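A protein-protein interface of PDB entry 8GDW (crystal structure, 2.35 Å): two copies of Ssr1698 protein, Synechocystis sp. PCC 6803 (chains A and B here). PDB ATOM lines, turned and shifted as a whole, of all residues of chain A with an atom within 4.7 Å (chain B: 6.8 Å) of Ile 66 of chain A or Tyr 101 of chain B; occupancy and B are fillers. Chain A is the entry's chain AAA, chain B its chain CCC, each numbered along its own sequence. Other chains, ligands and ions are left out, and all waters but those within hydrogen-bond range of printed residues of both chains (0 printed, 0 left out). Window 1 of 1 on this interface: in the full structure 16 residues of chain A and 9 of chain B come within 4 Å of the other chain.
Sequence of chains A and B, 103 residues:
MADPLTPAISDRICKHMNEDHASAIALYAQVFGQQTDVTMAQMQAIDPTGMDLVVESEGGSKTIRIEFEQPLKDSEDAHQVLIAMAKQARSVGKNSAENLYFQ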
ATOM      1  N   TYR A  28      30.660  -9.301 -29.334  1.00  0.00           N
ATOM      2  CA  TYR A  28      30.561  -7.853 -29.016  1.00  0.00           C
ATOM      3  C   TYR A  28      30.994  -7.632 -27.561  1.00  0.00           C
ATOM      4  O   TYR A  28      31.770  -6.705 -27.275  1.00  0.00           O
ATOM      5  CB  TYR A  28      29.136  -7.316 -29.182  1.00  0.00           C
ATOM      6  CG  TYR A  28      28.501  -7.368 -30.552  1.00  0.00           C
ATOM      7  CD1 TYR A  28      29.237  -7.338 -31.728  1.00  0.00           C
ATOM      8  CD2 TYR A  28      27.119  -7.364 -30.669  1.00  0.00           C
ATOM      9  CE1 TYR A  28      28.620  -7.345 -32.971  1.00  0.00           C
ATOM     10  CE2 TYR A  28      26.493  -7.373 -31.908  1.00  0.00           C
ATOM     11  CZ  TYR A  28      27.242  -7.369 -33.069  1.00  0.00           C
ATOM     12  OH  TYR A  28      26.607  -7.408 -34.282  1.00  0.00           O
ATOM     13  N   PHE A  32      34.433  -5.475 -28.066  1.00  0.00           N
ATOM     14  CA  PHE A  32      33.978  -4.085 -27.796  1.00  0.00           C
ATOM     15  C   PHE A  32      33.845  -3.874 -26.282  1.00  0.00           C
ATOM     16  O   PHE A  32      34.223  -2.808 -25.787  1.00  0.00           O
ATOM     17  CB  PHE A  32      32.701  -3.784 -28.579  1.00  0.00           C
ATOM     18  CG  PHE A  32      32.863  -3.874 -30.077  1.00  0.00           C
ATOM     19  CD1 PHE A  32      33.885  -3.196 -30.728  1.00  0.00           C
ATOM     20  CD2 PHE A  32      31.988  -4.625 -30.841  1.00  0.00           C
ATOM     21  CE1 PHE A  32      34.033  -3.280 -32.106  1.00  0.00           C
ATOM     22  CE2 PHE A  32      32.145  -4.718 -32.217  1.00  0.00           C
ATOM     23  CZ  PHE A  32      33.170  -4.049 -32.847  1.00  0.00           C
ATOM     24  N   GLY A  33      33.399  -4.899 -25.556  1.00  0.00           N
ATOM     25  CA  GLY A  33      33.065  -4.797 -24.123  1.00  0.00           C
ATOM     26  C   GLY A  33      34.166  -5.319 -23.223  1.00  0.00           C
ATOM     27  O   GLY A  33      33.951  -5.333 -22.002  1.00  0.00           O
ATOM     28  N   GLN A  34      35.312  -5.710 -23.787  1.00  0.00           N
ATOM     29  CA  GLN A  34      36.523  -6.102 -23.008  1.00  0.00           C
ATOM     30  C   GLN A  34      36.142  -7.074 -21.882  1.00  0.00           C
ATOM     31  O   GLN A  34      36.844  -7.062 -20.853  1.00  0.00           O
ATOM     32  CB  GLN A  34      37.205  -4.887 -22.368  1.00  0.00           C
ATOM     33  CG  GLN A  34      37.894  -3.946 -23.346  1.00  0.00           C
ATOM     34  CD  GLN A  34      38.292  -2.620 -22.726  1.00  0.00           C
ATOM     35  OE1 GLN A  34      38.043  -1.557 -23.284  1.00  0.00           O
ATOM     36  NE2 GLN A  34      38.928  -2.655 -21.564  1.00  0.00           N
ATOM     37  N   GLN A  35      35.078  -7.870 -22.052  1.00  0.00           N
ATOM     38  CA  GLN A  35      34.757  -9.017 -21.156  1.00  0.00           C
ATOM     39  C   GLN A  35      35.542 -10.224 -21.668  1.00  0.00           C
ATOM     40  O   GLN A  35      35.486 -10.456 -22.880  1.00  0.00           O
ATOM     41  CB  GLN A  35      33.270  -9.367 -21.196  1.00  0.00           C
ATOM     42  CG  GLN A  35      32.331  -8.189 -21.028  1.00  0.00           C
ATOM     43  CD  GLN A  35      32.502  -7.545 -19.679  1.00  0.00           C
ATOM     44  OE1 GLN A  35      32.288  -8.182 -18.651  1.00  0.00           O
ATOM     45  NE2 GLN A  35      32.874  -6.272 -19.685  1.00  0.00           N
ATOM     46  N   THR A  49      22.436   5.633 -31.029  1.00  0.00           N
ATOM     47  CA  THR A  49      23.812   5.945 -30.520  1.00  0.00           C
ATOM     48  C   THR A  49      24.502   4.724 -29.888  1.00  0.00           C
ATOM     49  O   THR A  49      25.693   4.839 -29.581  1.00  0.00           O
ATOM     50  CB  THR A  49      23.794   7.091 -29.499  1.00  0.00           C
ATOM     51  OG1 THR A  49      22.958   6.720 -28.401  1.00  0.00           O
ATOM     52  CG2 THR A  49      23.321   8.416 -30.063  1.00  0.00           C
ATOM     53  N   GLY A  50      23.816   3.597 -29.685  1.00  0.00           N
ATOM     54  CA  GLY A  50      24.454   2.416 -29.062  1.00  0.00           C
ATOM     55  C   GLY A  50      23.496   1.295 -28.702  1.00  0.00           C
ATOM     56  O   GLY A  50      22.285   1.430 -28.907  1.00  0.00           O
ATOM     57  N   MET A  51      24.046   0.231 -28.123  1.00  0.00           N
ATOM     58  CA  MET A  51      23.315  -1.005 -27.769  1.00  0.00           C
ATOM     59  C   MET A  51      23.668  -1.447 -26.355  1.00  0.00           C
ATOM     60  O   MET A  51      24.822  -1.309 -25.945  1.00  0.00           O
ATOM     61  CB  MET A  51      23.648  -2.132 -28.745  1.00  0.00           C
ATOM     62  CG  MET A  51      25.109  -2.339 -28.989  1.00  0.00           C
ATOM     63  SD  MET A  51      25.300  -3.813 -30.012  1.00  0.00           S
ATOM     64  CE  MET A  51      27.001  -3.706 -30.555  1.00  0.00           C
ATOM     65  N   LEU A  53      23.700  -4.536 -23.504  1.00  0.00           N
ATOM     66  CA  LEU A  53      23.990  -5.995 -23.509  1.00  0.00           C
ATOM     67  C   LEU A  53      23.903  -6.523 -22.072  1.00  0.00           C
ATOM     68  O   LEU A  53      24.324  -5.798 -21.186  1.00  0.00           O
ATOM     69  CB  LEU A  53      25.404  -6.189 -24.065  1.00  0.00           C
ATOM     70  CG  LEU A  53      25.514  -6.667 -25.503  1.00  0.00           C
ATOM     71  CD1 LEU A  53      24.483  -5.997 -26.391  1.00  0.00           C
ATOM     72  CD2 LEU A  53      26.921  -6.439 -26.024  1.00  0.00           C
ATOM     73  N   ILE A  64      26.153  -3.941 -19.870  1.00  0.00           N
ATOM     74  CA  ILE A  64      27.106  -2.980 -20.472  1.00  0.00           C
ATOM     75  C   ILE A  64      26.413  -2.267 -21.633  1.00  0.00           C
ATOM     76  O   ILE A  64      25.393  -2.764 -22.153  1.00  0.00           O
ATOM     77  CB  ILE A  64      28.381  -3.706 -20.914  1.00  0.00           C
ATOM     78  CG1 ILE A  64      28.205  -4.381 -22.268  1.00  0.00           C
ATOM     79  CG2 ILE A  64      28.837  -4.691 -19.851  1.00  0.00           C
ATOM     80  CD1 ILE A  64      29.482  -5.011 -22.795  1.00  0.00           C
ATOM     81  N   ARG A  65      26.971  -1.141 -22.026  1.00  0.00           N
ATOM     82  CA  ARG A  65      26.541  -0.418 -23.233  1.00  0.00           C
ATOM     83  C   ARG A  65      27.742  -0.222 -24.147  1.00  0.00           C
ATOM     84  O   ARG A  65      28.831   0.126 -23.651  1.00  0.00           O
ATOM     85  CB  ARG A  65      25.872   0.898 -22.849  1.00  0.00           C
ATOM     86  CG  ARG A  65      25.452   1.742 -24.042  1.00  0.00           C
ATOM     87  CD  ARG A  65      24.691   2.953 -23.549  1.00  0.00           C
ATOM     88  NE  ARG A  65      24.293   3.804 -24.646  1.00  0.00           N
ATOM     89  CZ  ARG A  65      23.222   3.600 -25.410  1.00  0.00           C
ATOM     90  NH1 ARG A  65      22.424   2.564 -25.202  1.00  0.00           N
ATOM     91  NH2 ARG A  65      22.945   4.445 -26.381  1.00  0.00           N
ATOM     92  N   ILE A  66      27.518  -0.420 -25.444  1.00  0.00           N
ATOM     93  CA  ILE A  66      28.520  -0.111 -26.497  1.00  0.00           C
ATOM     94  C   ILE A  66      27.990   1.020 -27.373  1.00  0.00           C
ATOM     95  O   ILE A  66      26.885   0.921 -27.935  1.00  0.00           O
ATOM     96  CB  ILE A  66      28.870  -1.384 -27.269  1.00  0.00           C
ATOM     97  CG1 ILE A  66      29.180  -2.502 -26.272  1.00  0.00           C
ATOM     98  CG2 ILE A  66      30.024  -1.134 -28.227  1.00  0.00           C
ATOM     99  CD1 ILE A  66      29.399  -3.840 -26.904  1.00  0.00           C
ATOM    100  N   GLU A  67      28.747   2.103 -27.431  1.00  0.00           N
ATOM    101  CA  GLU A  67      28.365   3.314 -28.196  1.00  0.00           C
ATOM    102  C   GLU A  67      28.972   3.189 -29.598  1.00  0.00           C
ATOM    103  O   GLU A  67      30.161   2.858 -29.709  1.00  0.00           O
ATOM    104  CB  GLU A  67      28.813   4.534 -27.401  1.00  0.00           C
ATOM    105  CG  GLU A  67      28.110   5.812 -27.813  1.00  0.00           C
ATOM    106  CD  GLU A  67      28.662   7.039 -27.118  1.00  0.00           C
ATOM    107  OE1 GLU A  67      29.559   7.677 -27.692  1.00  0.00           O
ATOM    108  OE2 GLU A  67      28.197   7.340 -26.007  1.00  0.00           O
ATOM    109  N   PHE A  68      28.152   3.339 -30.633  1.00  0.00           N
ATOM    110  CA  PHE A  68      28.602   3.324 -32.049  1.00  0.00           C
ATOM    111  C   PHE A  68      29.490   4.550 -32.306  1.00  0.00           C
ATOM    112  O   PHE A  68      29.300   5.579 -31.669  1.00  0.00           O
ATOM    113  CB  PHE A  68      27.400   3.309 -33.003  1.00  0.00           C
ATOM    114  CG  PHE A  68      26.381   2.236 -32.708  1.00  0.00           C
ATOM    115  CD1 PHE A  68      26.765   0.917 -32.570  1.00  0.00           C
ATOM    116  CD2 PHE A  68      25.043   2.548 -32.533  1.00  0.00           C
ATOM    117  CE1 PHE A  68      25.828  -0.067 -32.284  1.00  0.00           C
ATOM    118  CE2 PHE A  68      24.109   1.563 -32.244  1.00  0.00           C
ATOM    119  CZ  PHE A  68      24.502   0.259 -32.131  1.00  0.00           C
ATOM    120  N   SER B  96      23.179  -0.099 -17.447  1.00  0.00           N
ATOM    121  CA  SER B  96      24.013  -0.466 -18.628  1.00  0.00           C
ATOM    122  C   SER B  96      24.959   0.676 -19.024  1.00  0.00           C
ATOM    123  O   SER B  96      26.120   0.376 -19.415  1.00  0.00           O
ATOM    124  CB  SER B  96      23.133  -0.868 -19.788  1.00  0.00           C
ATOM    125  OG  SER B  96      22.421   0.252 -20.295  1.00  0.00           O
ATOM    126  N   GLU B  98      26.268   2.859 -17.217  1.00  0.00           N
ATOM    127  CA  GLU B  98      27.367   2.932 -16.216  1.00  0.00           C
ATOM    128  C   GLU B  98      28.591   2.197 -16.776  1.00  0.00           C
ATOM    129  O   GLU B  98      29.714   2.578 -16.411  1.00  0.00           O
ATOM    130  CB  GLU B  98      26.978   2.308 -14.864  1.00  0.00           C
ATOM    131  CG  GLU B  98      25.951   3.084 -14.030  1.00  0.00           C
ATOM    132  CD  GLU B  98      25.859   4.598 -14.208  1.00  0.00           C
ATOM    133  OE1 GLU B  98      26.763   5.315 -13.718  1.00  0.00           O
ATOM    134  OE2 GLU B  98      24.870   5.067 -14.824  1.00  0.00           O
ATOM    135  N   ASN B  99      28.392   1.136 -17.569  1.00  0.00           N
ATOM    136  CA  ASN B  99      29.516   0.346 -18.133  1.00  0.00           C
ATOM    137  C   ASN B  99      29.578   0.613 -19.635  1.00  0.00           C
ATOM    138  O   ASN B  99      29.359  -0.344 -20.422  1.00  0.00           O
ATOM    139  CB  ASN B  99      29.409  -1.134 -17.785  1.00  0.00           C
ATOM    140  CG  ASN B  99      29.158  -1.364 -16.314  1.00  0.00           C
ATOM    141  OD1 ASN B  99      29.330  -0.460 -15.511  1.00  0.00           O
ATOM    142  ND2 ASN B  99      28.733  -2.561 -15.954  1.00  0.00           N
ATOM    143  N   LEU B 100      29.911   1.864 -19.985  1.00  0.00           N
ATOM    144  CA  LEU B 100      29.956   2.412 -21.371  1.00  0.00           C
ATOM    145  C   LEU B 100      31.295   2.023 -22.013  1.00  0.00           C
ATOM    146  O   LEU B 100      32.335   2.196 -21.361  1.00  0.00           O
ATOM    147  CB  LEU B 100      29.832   3.932 -21.282  1.00  0.00           C
ATOM    148  CG  LEU B 100      29.055   4.662 -22.372  1.00  0.00           C
ATOM    149  CD1 LEU B 100      29.617   6.064 -22.557  1.00  0.00           C
ATOM    150  CD2 LEU B 100      29.041   3.919 -23.687  1.00  0.00           C
ATOM    151  N   TYR B 101      31.252   1.486 -23.225  1.00  0.00           N
ATOM    152  CA  TYR B 101      32.420   1.089 -24.043  1.00  0.00           C
ATOM    153  C   TYR B 101      32.211   1.764 -25.385  1.00  0.00           C
ATOM    154  O   TYR B 101      31.109   2.303 -25.541  1.00  0.00           O
ATOM    155  CB  TYR B 101      32.538  -0.437 -24.146  1.00  0.00           C
ATOM    156  CG  TYR B 101      32.886  -1.111 -22.843  1.00  0.00           C
ATOM    157  CD1 TYR B 101      31.907  -1.370 -21.896  1.00  0.00           C
ATOM    158  CD2 TYR B 101      34.198  -1.440 -22.528  1.00  0.00           C
ATOM    159  CE1 TYR B 101      32.219  -1.960 -20.681  1.00  0.00           C
ATOM    160  CE2 TYR B 101      34.530  -2.012 -21.307  1.00  0.00           C
ATOM    161  CZ  TYR B 101      33.537  -2.276 -20.382  1.00  0.00           C
ATOM    162  OH  TYR B 101      33.841  -2.848 -19.178  1.00  0.00           O
ATOM    163  N   PHE B 102      33.224   1.804 -26.257  1.00  0.00           N
ATOM    164  CA  PHE B 102      33.152   2.507 -27.566  1.00  0.00           C
ATOM    165  C   PHE B 102      33.584   1.529 -28.644  1.00  0.00           C
ATOM    166  O   PHE B 102      34.531   0.805 -28.372  1.00  0.00           O
ATOM    167  CB  PHE B 102      34.054   3.742 -27.563  1.00  0.00           C
ATOM    168  CG  PHE B 102      33.725   4.669 -26.433  1.00  0.00           C
ATOM    169  CD1 PHE B 102      32.771   5.655 -26.590  1.00  0.00           C
ATOM    170  CD2 PHE B 102      34.277   4.473 -25.182  1.00  0.00           C
ATOM    171  CE1 PHE B 102      32.404   6.456 -25.519  1.00  0.00           C
ATOM    172  CE2 PHE B 102      33.909   5.271 -24.116  1.00  0.00           C
ATOM    173  CZ  PHE B 102      32.966   6.257 -24.285  1.00  0.00           C
ATOM    174  N   GLN B 103      32.910   1.483 -29.795  1.00  0.00           N
ATOM    175  CA  GLN B 103      33.535   0.854 -30.987  1.00  0.00           C
ATOM    176  C   GLN B 103      34.556   1.866 -31.528  1.00  0.00           C
ATOM    177  O   GLN B 103      35.653   1.347 -31.683  1.00  0.00           O
ATOM    178  CB  GLN B 103      32.500   0.370 -32.013  1.00  0.00           C
ATOM    179  CG  GLN B 103      32.029   1.459 -32.954  1.00  0.00           C
ATOM    180  CD  GLN B 103      31.250   1.029 -34.172  1.00  0.00           C
ATOM    181  OE1 GLN B 103      30.223   1.631 -34.472  1.00  0.00           O
ATOM    182  NE2 GLN B 103      31.774   0.078 -34.932  1.00  0.00           N
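N of Arg 65 of chain A lies within hydrogen-bond range of O of Ser 96 of chain B, 3.1 Å away. The backbone NH of Arg 65 of chain A sits at hydrogen-bond distance from the backbone carbonyl oxygen of Asn 99 of chain B, at 3.0 Å. The backbone carbonyl oxygen (O) of Arg 65 of chain A is in hydrogen-bond range of the backbone NH (N) of Tyr 101 of chain B (2.8 Å). The backbone NH (N) of Glu 67 of chain A sits at hydrogen-bond distance from the backbone carbonyl oxygen (O) of Tyr 101 of chain B. O of Glu 67 of chain A lies within hydrogen-bond range of N of Gln 103 of chain B, 3.1 Å away.
The backbone carbonyl oxygen of Tyr 28 of chain A lies within hydrogen-bond range of the backbone NH of Gly 33 of chain A (3.0 Å). The backbone carbonyl oxygen (O) of Gly 33 of chain A lies within hydrogen-bond range of the side-chain amide nitrogen (NE2) of Gln 35 of chain A, 2.7 Å away. NH2 of Arg 65 of chain A is in hydrogen-bond range of OG1 of Thr 49 of chain A (3.0 Å). The backbone NH (N) of Phe 68 of chain A sits at hydrogen-bond distance from the backbone carbonyl oxygen (O) of Thr 49 of chain A, at 3.1 Å. The backbone carbonyl oxygen (O) of Met 51 of chain A is in hydrogen-bond range of the backbone NH (N) of Ile 66 of chain A. The backbone NH (N) of Leu 53 of chain A sits at hydrogen-bond distance from the backbone carbonyl oxygen (O) of Ile 64 of chain A (2.8 Å).
Among the printed residues, pairs that only touch across the chains: Phe 32 of chain A with Tyr 101 of chain B, Phe 68 of chain A with Gln 103 of chain B, Arg 65 of chain A with Leu 100 of chain B, Gly 33 of chain A with Tyr 101 of chain B, Ile 64 of chain A with Ser 96 of chain B, Ile 64 of chain A with Asn 99 of chain B, Gln 35 of chain A with Tyr 101 of chain B, Ile 66 of chain A with Tyr 101 of chain B, Glu 67 of chain A with Phe 102 of chain B, Glu 67 of chain A with Leu 100 of chain B, Gln 34 of chain A with Tyr 101 of chain B and Phe 32 of chain A with Gln 103 of chain B.
Of the printed residues of chain B, Gly 33 of chain A touches Tyr 101 (3.4 Å). Printed residues of chain B within 4 Å of Gln 35 of chain A: Tyr 101. Thr 49 of chain A touches none of the printed residues of chain B. Met 51 of chain A touches none of the printed residues of chain B. Printed residues of chain B within 4 Å of Ile 64 of chain A: Ser 96 (3.5 Å) and Asn 99 (3.5 Å). Of chain B, only Tyr 101 (3.7 Å) comes within 4 Å of Ile 66 of chain A. Of the printed residues of chain A, Ser 96 of chain B touches Ile 64 and Arg 65. Printed residues of chain A within 4 Å of Asn 99 of chain B: Ile 64 (3.5 Å) and Arg 65 (3.0 Å). Of the printed residues of chain A, Tyr 101 of chain B touches Phe 32, Gly 33, Gln 34, Gln 35, Arg 65, Ile 66 and Glu 67. The nearest residue of chain A that does not touch Tyr 101 of chain B is Ile 64 of chain A (4.2 Å).
Of the 14 printed residues of chain A, 9 touch a printed residue of chain B.
No position is printed for both chains. Of the 17 pairs that touch across the chains among the printed residues, none has its exchanged pair printed and touching as well.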
